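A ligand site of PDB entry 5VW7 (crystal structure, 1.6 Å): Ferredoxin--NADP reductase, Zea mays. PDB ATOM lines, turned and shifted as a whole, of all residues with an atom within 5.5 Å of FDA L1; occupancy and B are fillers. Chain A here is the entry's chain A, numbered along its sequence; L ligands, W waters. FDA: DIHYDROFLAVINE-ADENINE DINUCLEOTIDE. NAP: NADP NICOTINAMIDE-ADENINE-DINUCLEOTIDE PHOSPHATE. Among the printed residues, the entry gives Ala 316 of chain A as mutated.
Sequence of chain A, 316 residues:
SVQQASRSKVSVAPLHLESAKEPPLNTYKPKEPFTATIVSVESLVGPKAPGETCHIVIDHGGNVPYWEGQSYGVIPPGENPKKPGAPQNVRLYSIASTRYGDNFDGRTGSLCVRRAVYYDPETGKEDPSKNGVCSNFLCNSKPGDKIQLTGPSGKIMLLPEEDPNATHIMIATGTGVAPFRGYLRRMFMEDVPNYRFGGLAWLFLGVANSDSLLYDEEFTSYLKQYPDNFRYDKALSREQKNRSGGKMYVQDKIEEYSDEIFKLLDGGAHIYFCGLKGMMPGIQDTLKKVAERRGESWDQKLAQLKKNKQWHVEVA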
ATOM      1  N   SER A  71     -32.785   7.364 -12.150  1.00  0.00           N
ATOM      2  CA  SER A  71     -31.797   7.272 -13.203  1.00  0.00           C
ATOM      3  C   SER A  71     -31.262   5.846 -13.304  1.00  0.00           C
ATOM      4  O   SER A  71     -31.153   5.139 -12.303  1.00  0.00           O
ATOM      5  CB  SER A  71     -30.604   8.212 -12.968  1.00  0.00           C
ATOM      6  OG  SER A  71     -31.012   9.572 -13.025  1.00  0.00           O
ATOM      7  N   ARG A  91     -22.030   6.717 -16.490  1.00  0.00           N
ATOM      8  CA  ARG A  91     -22.794   7.912 -16.845  1.00  0.00           C
ATOM      9  C   ARG A  91     -24.251   7.686 -16.467  1.00  0.00           C
ATOM     10  O   ARG A  91     -24.816   6.617 -16.719  1.00  0.00           O
ATOM     11  CB  ARG A  91     -22.727   8.225 -18.343  1.00  0.00           C
ATOM     12  CG  ARG A  91     -21.475   8.912 -18.820  1.00  0.00           C
ATOM     13  CD  ARG A  91     -20.236   8.022 -18.814  1.00  0.00           C
ATOM     14  NE  ARG A  91     -19.221   8.638 -19.675  1.00  0.00           N
ATOM     15  CZ  ARG A  91     -17.939   8.289 -19.720  1.00  0.00           C
ATOM     16  NH1 ARG A  91     -17.488   7.295 -18.952  1.00  0.00           N
ATOM     17  NH2 ARG A  91     -17.110   8.923 -20.552  1.00  0.00           N
ATOM     18  N   LEU A  92     -24.879   8.700 -15.869  1.00  0.00           N
ATOM     19  CA  LEU A  92     -26.272   8.571 -15.460  1.00  0.00           C
ATOM     20  C   LEU A  92     -27.219   9.123 -16.520  1.00  0.00           C
ATOM     21  O   LEU A  92     -26.932  10.131 -17.177  1.00  0.00           O
ATOM     22  CB  LEU A  92     -26.519   9.322 -14.142  1.00  0.00           C
ATOM     23  CG  LEU A  92     -25.755   8.790 -12.939  1.00  0.00           C
ATOM     24  CD1 LEU A  92     -25.824   9.777 -11.799  1.00  0.00           C
ATOM     25  CD2 LEU A  92     -26.267   7.442 -12.500  1.00  0.00           C
ATOM     26  N   TYR A  93     -28.374   8.478 -16.654  1.00  0.00           N
ATOM     27  CA  TYR A  93     -29.426   8.899 -17.578  1.00  0.00           C
ATOM     28  C   TYR A  93     -30.767   8.823 -16.870  1.00  0.00           C
ATOM     29  O   TYR A  93     -31.121   7.784 -16.313  1.00  0.00           O
ATOM     30  CB  TYR A  93     -29.406   8.013 -18.855  1.00  0.00           C
ATOM     31  CG  TYR A  93     -28.140   8.276 -19.636  1.00  0.00           C
ATOM     32  CD1 TYR A  93     -28.021   9.387 -20.451  1.00  0.00           C
ATOM     33  CD2 TYR A  93     -27.025   7.468 -19.476  1.00  0.00           C
ATOM     34  CE1 TYR A  93     -26.830   9.708 -21.103  1.00  0.00           C
ATOM     35  CE2 TYR A  93     -25.818   7.774 -20.108  1.00  0.00           C
ATOM     36  CZ  TYR A  93     -25.725   8.903 -20.934  1.00  0.00           C
ATOM     37  OH  TYR A  93     -24.544   9.235 -21.571  1.00  0.00           O
ATOM     38  N   SER A  94     -31.531   9.917 -16.933  1.00  0.00           N
ATOM     39  CA  SER A  94     -32.852   9.933 -16.322  1.00  0.00           C
ATOM     40  C   SER A  94     -33.800   9.058 -17.109  1.00  0.00           C
ATOM     41  O   SER A  94     -33.945   9.211 -18.320  1.00  0.00           O
ATOM     42  CB  SER A  94     -33.418  11.349 -16.246  1.00  0.00           C
ATOM     43  OG  SER A  94     -32.684  12.139 -15.336  1.00  0.00           O
ATOM     44  N   CYS A 112     -33.590   9.005 -22.989  1.00  0.00           N
ATOM     45  CA  CYS A 112     -33.708  10.141 -23.905  1.00  0.00           C
ATOM     46  C   CYS A 112     -32.340  10.781 -23.912  1.00  0.00           C
ATOM     47  O   CYS A 112     -31.968  11.426 -22.920  1.00  0.00           O
ATOM     48  CB  CYS A 112     -34.800  11.088 -23.423  1.00  0.00           C
ATOM     49  SG  CYS A 112     -35.029  12.537 -24.412  1.00  0.00           S
ATOM     50  N   VAL A 113     -31.562  10.576 -24.966  1.00  0.00           N
ATOM     51  CA  VAL A 113     -30.111  10.808 -24.930  1.00  0.00           C
ATOM     52  C   VAL A 113     -29.704  11.801 -26.023  1.00  0.00           C
ATOM     53  O   VAL A 113     -29.924  11.538 -27.203  1.00  0.00           O
ATOM     54  CB  VAL A 113     -29.349   9.484 -25.110  1.00  0.00           C
ATOM     55  CG1 VAL A 113     -27.830   9.722 -25.152  1.00  0.00           C
ATOM     56  CG2 VAL A 113     -29.712   8.497 -24.018  1.00  0.00           C
ATOM     57  N   ARG A 114     -29.089  12.928 -25.626  1.00  0.00           N
ATOM     58  CA  ARG A 114     -28.507  13.876 -26.569  1.00  0.00           C
ATOM     59  C   ARG A 114     -27.098  13.422 -26.916  1.00  0.00           C
ATOM     60  O   ARG A 114     -26.280  13.174 -26.036  1.00  0.00           O
ATOM     61  CB  ARG A 114     -28.491  15.285 -25.956  1.00  0.00           C
ATOM     62  CG  ARG A 114     -27.765  16.351 -26.800  1.00  0.00           C
ATOM     63  CD  ARG A 114     -28.461  16.633 -28.114  1.00  0.00           C
ATOM     64  NE  ARG A 114     -27.671  17.575 -28.920  1.00  0.00           N
ATOM     65  CZ  ARG A 114     -27.879  18.894 -28.975  1.00  0.00           C
ATOM     66  NH1 ARG A 114     -27.078  19.639 -29.724  1.00  0.00           N
ATOM     67  NH2 ARG A 114     -28.870  19.460 -28.300  1.00  0.00           N
ATOM     68  N   ALA A 116     -23.503  14.000 -27.567  1.00  0.00           N
ATOM     69  CA  ALA A 116     -22.524  15.049 -27.292  1.00  0.00           C
ATOM     70  C   ALA A 116     -21.481  15.037 -28.406  1.00  0.00           C
ATOM     71  O   ALA A 116     -20.735  14.055 -28.554  1.00  0.00           O
ATOM     72  CB  ALA A 116     -21.897  14.823 -25.915  1.00  0.00           C
ATOM     73  N   VAL A 117     -21.446  16.106 -29.213  1.00  0.00           N
ATOM     74  CA  VAL A 117     -20.566  16.215 -30.375  1.00  0.00           C
ATOM     75  C   VAL A 117     -19.685  17.452 -30.226  1.00  0.00           C
ATOM     76  O   VAL A 117     -20.159  18.515 -29.815  1.00  0.00           O
ATOM     77  CB  VAL A 117     -21.369  16.260 -31.696  1.00  0.00           C
ATOM     78  CG1 VAL A 117     -20.438  16.415 -32.910  1.00  0.00           C
ATOM     79  CG2 VAL A 117     -22.191  14.988 -31.858  1.00  0.00           C
ATOM     80  N   TYR A 118     -18.391  17.307 -30.530  1.00  0.00           N
ATOM     81  CA  TYR A 118     -17.420  18.390 -30.397  1.00  0.00           C
ATOM     82  C   TYR A 118     -17.237  19.130 -31.722  1.00  0.00           C
ATOM     83  O   TYR A 118     -17.039  18.499 -32.760  1.00  0.00           O
ATOM     84  CB  TYR A 118     -16.057  17.835 -29.954  1.00  0.00           C
ATOM     85  CG  TYR A 118     -15.000  18.926 -29.884  1.00  0.00           C
ATOM     86  CD1 TYR A 118     -14.223  19.232 -30.989  1.00  0.00           C
ATOM     87  CD2 TYR A 118     -14.787  19.653 -28.711  1.00  0.00           C
ATOM     88  CE1 TYR A 118     -13.263  20.242 -30.928  1.00  0.00           C
ATOM     89  CE2 TYR A 118     -13.826  20.663 -28.651  1.00  0.00           C
ATOM     90  CZ  TYR A 118     -13.073  20.942 -29.756  1.00  0.00           C
ATOM     91  OH  TYR A 118     -12.120  21.940 -29.698  1.00  0.00           O
ATOM     92  N   SER A 129     -12.915  12.301 -31.924  1.00  0.00           N
ATOM     93  CA  SER A 129     -12.208  11.819 -30.744  1.00  0.00           C
ATOM     94  C   SER A 129     -12.567  12.611 -29.497  1.00  0.00           C
ATOM     95  O   SER A 129     -12.281  12.143 -28.382  1.00  0.00           O
ATOM     96  CB  SER A 129     -10.695  11.876 -30.963  1.00  0.00           C
ATOM     97  OG  SER A 129     -10.204  13.207 -30.862  1.00  0.00           O
ATOM     98  N   LYS A 130     -13.190  13.771 -29.655  1.00  0.00           N
ATOM     99  CA  LYS A 130     -13.644  14.571 -28.530  1.00  0.00           C
ATOM    100  C   LYS A 130     -15.152  14.506 -28.334  1.00  0.00           C
ATOM    101  O   LYS A 130     -15.699  15.249 -27.524  1.00  0.00           O
ATOM    102  CB  LYS A 130     -13.190  16.000 -28.724  1.00  0.00           C
ATOM    103  CG  LYS A 130     -11.655  16.138 -28.732  1.00  0.00           C
ATOM    104  CD  LYS A 130     -11.228  17.581 -28.996  1.00  0.00           C
ATOM    105  CE  LYS A 130      -9.712  17.669 -28.993  1.00  0.00           C
ATOM    106  NZ  LYS A 130      -9.232  19.073 -29.182  1.00  0.00           N
ATOM    107  N   ASN A 131     -15.828  13.637 -29.069  1.00  0.00           N
ATOM    108  CA  ASN A 131     -17.247  13.428 -28.855  1.00  0.00           C
ATOM    109  C   ASN A 131     -17.483  12.711 -27.517  1.00  0.00           C
ATOM    110  O   ASN A 131     -16.588  12.111 -26.941  1.00  0.00           O
ATOM    111  CB  ASN A 131     -17.826  12.636 -30.032  1.00  0.00           C
ATOM    112  CG  ASN A 131     -17.948  13.469 -31.327  1.00  0.00           C
ATOM    113  OD1 ASN A 131     -17.620  14.670 -31.377  1.00  0.00           O
ATOM    114  ND2 ASN A 131     -18.449  12.818 -32.396  1.00  0.00           N
ATOM    115  N   GLY A 132     -18.700  12.805 -26.991  1.00  0.00           N
ATOM    116  CA  GLY A 132     -18.997  12.148 -25.724  1.00  0.00           C
ATOM    117  C   GLY A 132     -19.067  10.633 -25.934  1.00  0.00           C
ATOM    118  O   GLY A 132     -19.710  10.156 -26.872  1.00  0.00           O
ATOM    119  N   VAL A 133     -18.429   9.876 -25.033  1.00  0.00           N
ATOM    120  CA  VAL A 133     -18.322   8.419 -25.240  1.00  0.00           C
ATOM    121  C   VAL A 133     -19.675   7.732 -25.089  1.00  0.00           C
ATOM    122  O   VAL A 133     -20.106   6.984 -25.975  1.00  0.00           O
ATOM    123  CB  VAL A 133     -17.288   7.809 -24.288  1.00  0.00           C
ATOM    124  CG1 VAL A 133     -17.246   6.274 -24.455  1.00  0.00           C
ATOM    125  CG2 VAL A 133     -15.934   8.426 -24.561  1.00  0.00           C
ATOM    126  N   CYS A 134     -20.311   7.912 -23.932  1.00  0.00           N
ATOM    127  CA  CYS A 134     -21.493   7.106 -23.636  1.00  0.00           C
ATOM    128  C   CYS A 134     -22.696   7.535 -24.464  1.00  0.00           C
ATOM    129  O   CYS A 134     -23.494   6.694 -24.912  1.00  0.00           O
ATOM    130  CB  CYS A 134     -21.841   7.174 -22.146  1.00  0.00           C
ATOM    131  SG  CYS A 134     -22.849   5.773 -21.616  1.00  0.00           S
ATOM    132  N   SER A 135     -22.858   8.835 -24.699  1.00  0.00           N
ATOM    133  CA  SER A 135     -24.041   9.273 -25.422  1.00  0.00           C
ATOM    134  C   SER A 135     -24.016   8.783 -26.877  1.00  0.00           C
ATOM    135  O   SER A 135     -25.062   8.367 -27.401  1.00  0.00           O
ATOM    136  CB  SER A 135     -24.196  10.793 -25.335  1.00  0.00           C
ATOM    137  OG  SER A 135     -23.112  11.484 -25.939  1.00  0.00           O
ATOM    138  N   ASN A 136     -22.844   8.825 -27.520  1.00  0.00           N
ATOM    139  CA  ASN A 136     -22.740   8.309 -28.882  1.00  0.00           C
ATOM    140  C   ASN A 136     -22.779   6.798 -28.912  1.00  0.00           C
ATOM    141  O   ASN A 136     -23.393   6.219 -29.813  1.00  0.00           O
ATOM    142  CB  ASN A 136     -21.487   8.882 -29.554  1.00  0.00           C
ATOM    143  CG  ASN A 136     -21.676  10.360 -29.875  1.00  0.00           C
ATOM    144  OD1 ASN A 136     -22.403  10.722 -30.805  1.00  0.00           O
ATOM    145  ND2 ASN A 136     -21.083  11.224 -29.064  1.00  0.00           N
ATOM    146  N   THR A 175     -33.271  17.250 -23.129  1.00  0.00           N
ATOM    147  CA  THR A 175     -33.485  15.916 -22.596  1.00  0.00           C
ATOM    148  C   THR A 175     -33.863  15.912 -21.117  1.00  0.00           C
ATOM    149  O   THR A 175     -34.225  14.859 -20.592  1.00  0.00           O
ATOM    150  CB  THR A 175     -32.232  15.042 -22.806  1.00  0.00           C
ATOM    151  OG1 THR A 175     -31.084  15.702 -22.252  1.00  0.00           O
ATOM    152  CG2 THR A 175     -31.992  14.786 -24.283  1.00  0.00           C
ATOM    153  N   ALA A 178     -37.030  14.068 -19.795  1.00  0.00           N
ATOM    154  CA  ALA A 178     -37.105  12.619 -19.552  1.00  0.00           C
ATOM    155  C   ALA A 178     -37.979  12.197 -18.363  1.00  0.00           C
ATOM    156  O   ALA A 178     -38.916  11.406 -18.537  1.00  0.00           O
ATOM    157  CB  ALA A 178     -35.693  12.071 -19.387  1.00  0.00           C
ATOM    158  N   GLU A 314     -32.970  18.670 -10.492  1.00  0.00           N
ATOM    159  CA  GLU A 314     -31.901  17.770 -10.923  1.00  0.00           C
ATOM    160  C   GLU A 314     -31.424  18.250 -12.295  1.00  0.00           C
ATOM    161  O   GLU A 314     -32.122  18.074 -13.301  1.00  0.00           O
ATOM    162  CB  GLU A 314     -32.392  16.324 -10.959  1.00  0.00           C
ATOM    163  CG  GLU A 314     -31.445  15.309 -10.333  1.00  0.00           C
ATOM    164  CD  GLU A 314     -31.946  13.875 -10.483  1.00  0.00           C
ATOM    165  OE1 GLU A 314     -32.170  13.461 -11.618  1.00  0.00           O
ATOM    166  OE2 GLU A 314     -32.131  13.179  -9.459  1.00  0.00           O
ATOM    167  N   VAL A 315     -30.238  18.892 -12.332  1.00  0.00           N
ATOM    168  CA  VAL A 315     -29.700  19.474 -13.566  1.00  0.00           C
ATOM    169  C   VAL A 315     -28.231  19.105 -13.669  1.00  0.00           C
ATOM    170  O   VAL A 315     -27.591  18.727 -12.683  1.00  0.00           O
ATOM    171  CB  VAL A 315     -29.879  20.997 -13.632  1.00  0.00           C
ATOM    172  CG1 VAL A 315     -31.351  21.354 -13.708  1.00  0.00           C
ATOM    173  CG2 VAL A 315     -29.233  21.674 -12.428  1.00  0.00           C
ATOM    174  N   ALA A 316     -27.696  19.211 -14.882  1.00  0.00           N
ATOM    175  CA  ALA A 316     -26.288  18.860 -15.099  1.00  0.00           C
ATOM    176  C   ALA A 316     -25.721  19.570 -16.295  1.00  0.00           C
ATOM    177  O   ALA A 316     -26.449  20.227 -17.050  1.00  0.00           O
ATOM    178  CB  ALA A 316     -26.147  17.358 -15.277  1.00  0.00           C
ATOM    179  OXT ALA A 316     -24.508  19.467 -16.550  1.00  0.00           O
HETATM  180  PA  FDA L   1     -18.062  12.231 -22.005  1.00  0.00           P
HETATM  181  O1A FDA L   1     -17.220  11.288 -22.823  1.00  0.00           O
HETATM  182  O2A FDA L   1     -18.198  12.049 -20.522  1.00  0.00           O
HETATM  183  O5B FDA L   1     -17.534  13.712 -22.351  1.00  0.00           O
HETATM  184  C5B FDA L   1     -18.109  14.800 -21.612  1.00  0.00           C
HETATM  185  C4B FDA L   1     -18.112  16.020 -22.503  1.00  0.00           C
HETATM  186  O4B FDA L   1     -16.761  16.404 -22.789  1.00  0.00           O
HETATM  187  C3B FDA L   1     -18.769  15.803 -23.857  1.00  0.00           C
HETATM  188  O3B FDA L   1     -19.517  16.976 -24.198  1.00  0.00           O
HETATM  189  C2B FDA L   1     -17.589  15.656 -24.810  1.00  0.00           C
HETATM  190  O2B FDA L   1     -17.886  16.017 -26.164  1.00  0.00           O
HETATM  191  C1B FDA L   1     -16.584  16.604 -24.191  1.00  0.00           C
HETATM  192  N9A FDA L   1     -15.177  16.310 -24.483  1.00  0.00           N
HETATM  193  C8A FDA L   1     -14.555  15.119 -24.463  1.00  0.00           C
HETATM  194  N7A FDA L   1     -13.230  15.275 -24.756  1.00  0.00           N
HETATM  195  C5A FDA L   1     -13.020  16.573 -24.964  1.00  0.00           C
HETATM  196  C6A FDA L   1     -11.875  17.437 -25.308  1.00  0.00           C
HETATM  197  N6A FDA L   1     -10.668  16.891 -25.487  1.00  0.00           N
HETATM  198  N1A FDA L   1     -12.099  18.760 -25.419  1.00  0.00           N
HETATM  199  C2A FDA L   1     -13.312  19.318 -25.241  1.00  0.00           C
HETATM  200  N3A FDA L   1     -14.414  18.593 -24.922  1.00  0.00           N
HETATM  201  C4A FDA L   1     -14.291  17.253 -24.787  1.00  0.00           C
HETATM  202  N1  FDA L   1     -27.905  13.374 -20.508  1.00  0.00           N
HETATM  203  C2  FDA L   1     -28.869  13.064 -21.398  1.00  0.00           C
HETATM  204  O2  FDA L   1     -28.673  13.293 -22.622  1.00  0.00           O
HETATM  205  N3  FDA L   1     -30.043  12.536 -21.032  1.00  0.00           N
HETATM  206  C4  FDA L   1     -30.362  12.264 -19.755  1.00  0.00           C
HETATM  207  O4  FDA L   1     -31.445  11.747 -19.438  1.00  0.00           O
HETATM  208  C4X FDA L   1     -29.369  12.559 -18.711  1.00  0.00           C
HETATM  209  N5  FDA L   1     -29.629  12.327 -17.395  1.00  0.00           N
HETATM  210  C5X FDA L   1     -28.682  12.662 -16.489  1.00  0.00           C
HETATM  211  C6  FDA L   1     -28.957  12.481 -15.127  1.00  0.00           C
HETATM  212  C7  FDA L   1     -28.045  12.858 -14.150  1.00  0.00           C
HETATM  213  C7M FDA L   1     -28.386  12.650 -12.697  1.00  0.00           C
HETATM  214  C8  FDA L   1     -26.774  13.457 -14.544  1.00  0.00           C
HETATM  215  C8M FDA L   1     -25.779  13.871 -13.504  1.00  0.00           C
HETATM  216  C9  FDA L   1     -26.490  13.652 -15.874  1.00  0.00           C
HETATM  217  C9A FDA L   1     -27.392  13.264 -16.867  1.00  0.00           C
HETATM  218  N10 FDA L   1     -27.100  13.420 -18.245  1.00  0.00           N
HETATM  219  C10 FDA L   1     -28.087  13.135 -19.187  1.00  0.00           C
HETATM  220  C1' FDA L   1     -25.724  13.623 -18.719  1.00  0.00           C
HETATM  221  C2' FDA L   1     -25.054  12.265 -18.952  1.00  0.00           C
HETATM  222  O2' FDA L   1     -24.853  11.603 -17.701  1.00  0.00           O
HETATM  223  C3' FDA L   1     -23.673  12.420 -19.593  1.00  0.00           C
HETATM  224  O3' FDA L   1     -22.834  13.326 -18.831  1.00  0.00           O
HETATM  225  C4' FDA L   1     -23.748  12.920 -21.025  1.00  0.00           C
HETATM  226  O4' FDA L   1     -24.491  11.975 -21.804  1.00  0.00           O
HETATM  227  C5' FDA L   1     -22.360  13.041 -21.638  1.00  0.00           C
HETATM  228  O5' FDA L   1     -21.653  11.808 -21.423  1.00  0.00           O
HETATM  229  P   FDA L   1     -20.694  11.174 -22.553  1.00  0.00           P
HETATM  230  O1P FDA L   1     -20.100   9.932 -21.967  1.00  0.00           O
HETATM  231  O2P FDA L   1     -21.380  11.134 -23.893  1.00  0.00           O
HETATM  232  O3P FDA L   1     -19.540  12.310 -22.672  1.00  0.00           O
HETATM  233  PA  NAP L   2     -29.891  21.873 -25.606  1.00  0.00           P
HETATM  234  O1A NAP L   2     -30.447  21.728 -27.005  1.00  0.00           O
HETATM  235  O2A NAP L   2     -28.442  22.250 -25.396  1.00  0.00           O
HETATM  236  O5B NAP L   2     -30.756  22.998 -24.861  1.00  0.00           O
HETATM  237  C5B NAP L   2     -32.164  22.832 -24.682  1.00  0.00           C
HETATM  238  C4B NAP L   2     -32.774  24.220 -24.707  1.00  0.00           C
HETATM  239  O4B NAP L   2     -32.313  24.997 -23.593  1.00  0.00           O
HETATM  240  C3B NAP L   2     -32.360  24.977 -25.954  1.00  0.00           C
HETATM  241  O3B NAP L   2     -33.434  25.727 -26.504  1.00  0.00           O
HETATM  242  C2B NAP L   2     -31.342  25.986 -25.476  1.00  0.00           C
HETATM  243  O2B NAP L   2     -31.305  27.135 -26.302  1.00  0.00           O
HETATM  244  C1B NAP L   2     -31.920  26.248 -24.106  1.00  0.00           C
HETATM  245  N9A NAP L   2     -30.952  26.940 -23.230  1.00  0.00           N
HETATM  246  C8A NAP L   2     -29.610  27.097 -23.406  1.00  0.00           C
HETATM  247  N7A NAP L   2     -29.099  27.853 -22.389  1.00  0.00           N
HETATM  248  C5A NAP L   2     -30.122  28.166 -21.575  1.00  0.00           C
HETATM  249  C6A NAP L   2     -30.293  28.934 -20.333  1.00  0.00           C
HETATM  250  N6A NAP L   2     -29.224  29.525 -19.736  1.00  0.00           N
HETATM  251  N1A NAP L   2     -31.535  29.039 -19.824  1.00  0.00           N
HETATM  252  C2A NAP L   2     -32.615  28.468 -20.398  1.00  0.00           C
HETATM  253  N3A NAP L   2     -32.529  27.750 -21.538  1.00  0.00           N
HETATM  254  C4A NAP L   2     -31.341  27.589 -22.146  1.00  0.00           C
HETATM  255  O3  NAP L   2     -30.356  20.650 -24.669  1.00  0.00           O
HETATM  256  PN  NAP L   2     -29.726  19.199 -24.429  1.00  0.00           P
HETATM  257  O1N NAP L   2     -28.465  19.062 -25.221  1.00  0.00           O
HETATM  258  O2N NAP L   2     -30.858  18.221 -24.492  1.00  0.00           O
HETATM  259  O5D NAP L   2     -29.215  19.397 -22.943  1.00  0.00           O
HETATM  260  C5D NAP L   2     -29.957  19.049 -21.780  1.00  0.00           C
HETATM  261  C4D NAP L   2     -28.866  18.716 -20.782  1.00  0.00           C
HETATM  262  O4D NAP L   2     -29.461  18.503 -19.524  1.00  0.00           O
HETATM  263  C3D NAP L   2     -28.112  17.440 -21.139  1.00  0.00           C
HETATM  264  O3D NAP L   2     -27.005  17.729 -22.009  1.00  0.00           O
HETATM  265  C2D NAP L   2     -27.693  16.926 -19.784  1.00  0.00           C
HETATM  266  O2D NAP L   2     -26.374  17.382 -19.433  1.00  0.00           O
HETATM  267  C1D NAP L   2     -28.669  17.575 -18.804  1.00  0.00           C
HETATM  268  N1N NAP L   2     -29.620  16.639 -18.242  1.00  0.00           N
HETATM  269  C2N NAP L   2     -29.643  16.447 -16.941  1.00  0.00           C
HETATM  270  C3N NAP L   2     -30.555  15.580 -16.378  1.00  0.00           C
HETATM  271  C7N NAP L   2     -30.488  15.404 -14.889  1.00  0.00           C
HETATM  272  O7N NAP L   2     -29.662  16.029 -14.209  1.00  0.00           O
HETATM  273  N7N NAP L   2     -31.346  14.574 -14.300  1.00  0.00           N
HETATM  274  C4N NAP L   2     -31.469  14.870 -17.207  1.00  0.00           C
HETATM  275  C5N NAP L   2     -31.420  15.119 -18.576  1.00  0.00           C
HETATM  276  C6N NAP L   2     -30.501  16.010 -19.071  1.00  0.00           C
HETATM  277  P2B NAP L   2     -29.999  27.506 -27.199  1.00  0.00           P
HETATM  278  O1X NAP L   2     -29.235  26.239 -27.500  1.00  0.00           O
HETATM  279  O2X NAP L   2     -29.185  28.474 -26.373  1.00  0.00           O
HETATM  280  O3X NAP L   2     -30.673  28.140 -28.387  1.00  0.00           O
HETATM  281  O   HOH W   1     -12.988  19.872 -21.875  1.00  0.00           O
HETATM  282  O   HOH W   2     -16.165  12.116 -18.800  1.00  0.00           O
HETATM  283  O   HOH W   3     -14.641  11.772 -23.410  1.00  0.00           O
HETATM  284  O   HOH W   4     -11.302  13.251 -25.103  1.00  0.00           O
HETATM  285  O   HOH W   5     -21.929  16.412 -22.539  1.00  0.00           O
HETATM  286  O   HOH W   6     -32.486   9.469 -20.498  1.00  0.00           O
HETATM  287  O   HOH W   7     -26.117  13.513 -23.430  1.00  0.00           O
HETATM  288  O   HOH W   8     -23.189  14.963 -16.642  1.00  0.00           O
HETATM  289  O   HOH W   9     -23.659  16.667 -18.842  1.00  0.00           O
HETATM  290  O   HOH W  10     -19.816  18.435 -26.858  1.00  0.00           O
HETATM  291  O   HOH W  11     -10.198  20.364 -26.855  1.00  0.00           O
HETATM  292  O   HOH W  12     -20.121  13.021 -18.764  1.00  0.00           O
HETATM  293  O   HOH W  13     -23.124  11.267 -15.674  1.00  0.00           O
HETATM  294  O   HOH W  14     -16.535  20.319 -25.020  1.00  0.00           O
HETATM  295  O   HOH W  15     -14.221  16.163 -20.695  1.00  0.00           O
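The backbone NH of Leu 92 sits at hydrogen-bond distance from an oxygen (O2') of FDA L1, at 3.4 Å.
The backbone carbonyl oxygen (O) of Leu 92 lies within hydrogen-bond range of an oxygen (O2') of FDA L1, at 2.6 Å.
An oxygen (O2B) of FDA L1 is in hydrogen-bond range of the backbone carbonyl oxygen of Lys 130, at 2.7 Å.
N of Ser 135 sits at hydrogen-bond distance from O2P of FDA L1, at 2.8 Å.
O2P of FDA L1 sits at hydrogen-bond distance from OG of Ser 135 (2.7 Å).
The side-chain hydroxyl (OH) of Tyr 93 lies within hydrogen-bond range of an oxygen (O4') of FDA L1, 2.8 Å away.
O1P of FDA L1 lies within salt-bridge range of NE of Arg 91, at 2.8 Å.
The backbone NH of Cys 134 sits at hydrogen-bond distance from an oxygen (O1P) of FDA L1 (2.8 Å).
An oxygen (O1A) of FDA L1 is in hydrogen-bond range of the backbone NH (N) of Val 133.
The backbone carbonyl oxygen (O) of Cys 112 lies within hydrogen-bond range of a nitrogen (N3) of FDA L1 (2.9 Å).
The backbone NH (N) of Arg 114 lies within hydrogen-bond range of an oxygen (O2) of FDA L1, 3.1 Å away.
An oxygen (O4) of FDA L1 sits at hydrogen-bond distance from the backbone NH (N) of Ser 94 (3.1 Å).
N of Gly 132 sits at hydrogen-bond distance from O2B of FDA L1 (3.4 Å).
OG1 of Thr 175 is in hydrogen-bond range of O2 of FDA L1 (3.4 Å).
NH2 of Arg 114 is in salt-bridge range of O1A of NAP L2 (3.1 Å).
OG of Ser 94 sits at hydrogen-bond distance from N7N of NAP L2 (3.0 Å).
The backbone NH (N) of Thr 175 lies within hydrogen-bond range of an oxygen (O2N) of NAP L2 (2.9 Å).
An oxygen (O2N) of NAP L2 lies close to the side-chain hydroxyl (OG1) of Thr 175.
OE1 of Glu 314 is in hydrogen-bond range of N7N of NAP L2 (3.0 Å).
N of Val 315 lies close to O7N of NAP L2 (3.5 Å).
The side-chain hydroxyl (OG) of Ser 135 is in hydrogen-bond range of the backbone NH (N) of Ala 116 (3.0 Å).
N of Gly 132 sits at hydrogen-bond distance from O of Ala 116 (2.9 Å).
The backbone carbonyl oxygen (O) of Gly 132 lies within hydrogen-bond range of the side-chain amide nitrogen (ND2) of Asn 136, at 2.8 Å.
The side-chain amide oxygen (OD1) of Asn 131 sits at hydrogen-bond distance from the backbone NH (N) of Tyr 118, at 2.9 Å.
The side-chain amide nitrogen (ND2) of Asn 136 is in hydrogen-bond range of the backbone carbonyl oxygen (O) of Ala 116, 2.9 Å away.
Merely in contact with FDA L1: Val 113 (3.7 Å), Ala 116 (3.6 Å), Tyr 118 (3.7 Å), Asn 131 (3.6 Å) and Ala 316 (3.8 Å).
The nearest printed residue that does not touch FDA L1 is Glu 314 (4.02 Å).
Water W13 lies within hydrogen-bond range of an oxygen (O2') of FDA L1 (2.7 Å) and the backbone NH (N) of Leu 92 (3.1 Å).
Water W7 bridges the backbone carbonyl oxygen of Arg 114 (2.6 Å) and an oxygen (O2) of FDA L1 (2.7 Å).
Water W6 lies within hydrogen-bond range of the backbone carbonyl oxygen of Ser 94 (2.6 Å), an oxygen (O4) of FDA L1 (2.7 Å) and the backbone NH of Cys 112 (2.8 Å).
Water W11 bridges the side-chain amino group (NZ) of Lys 130 and a nitrogen (N1A) of FDA L1.
Water W10 lies within hydrogen-bond range of O of Val 117 (3.0 Å) and O3B of FDA L1 (3.0 Å).
Water W9 lies within hydrogen-bond range of O2D of NAP L2 (2.9 Å) and O3' of FDA L1 (3.4 Å).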
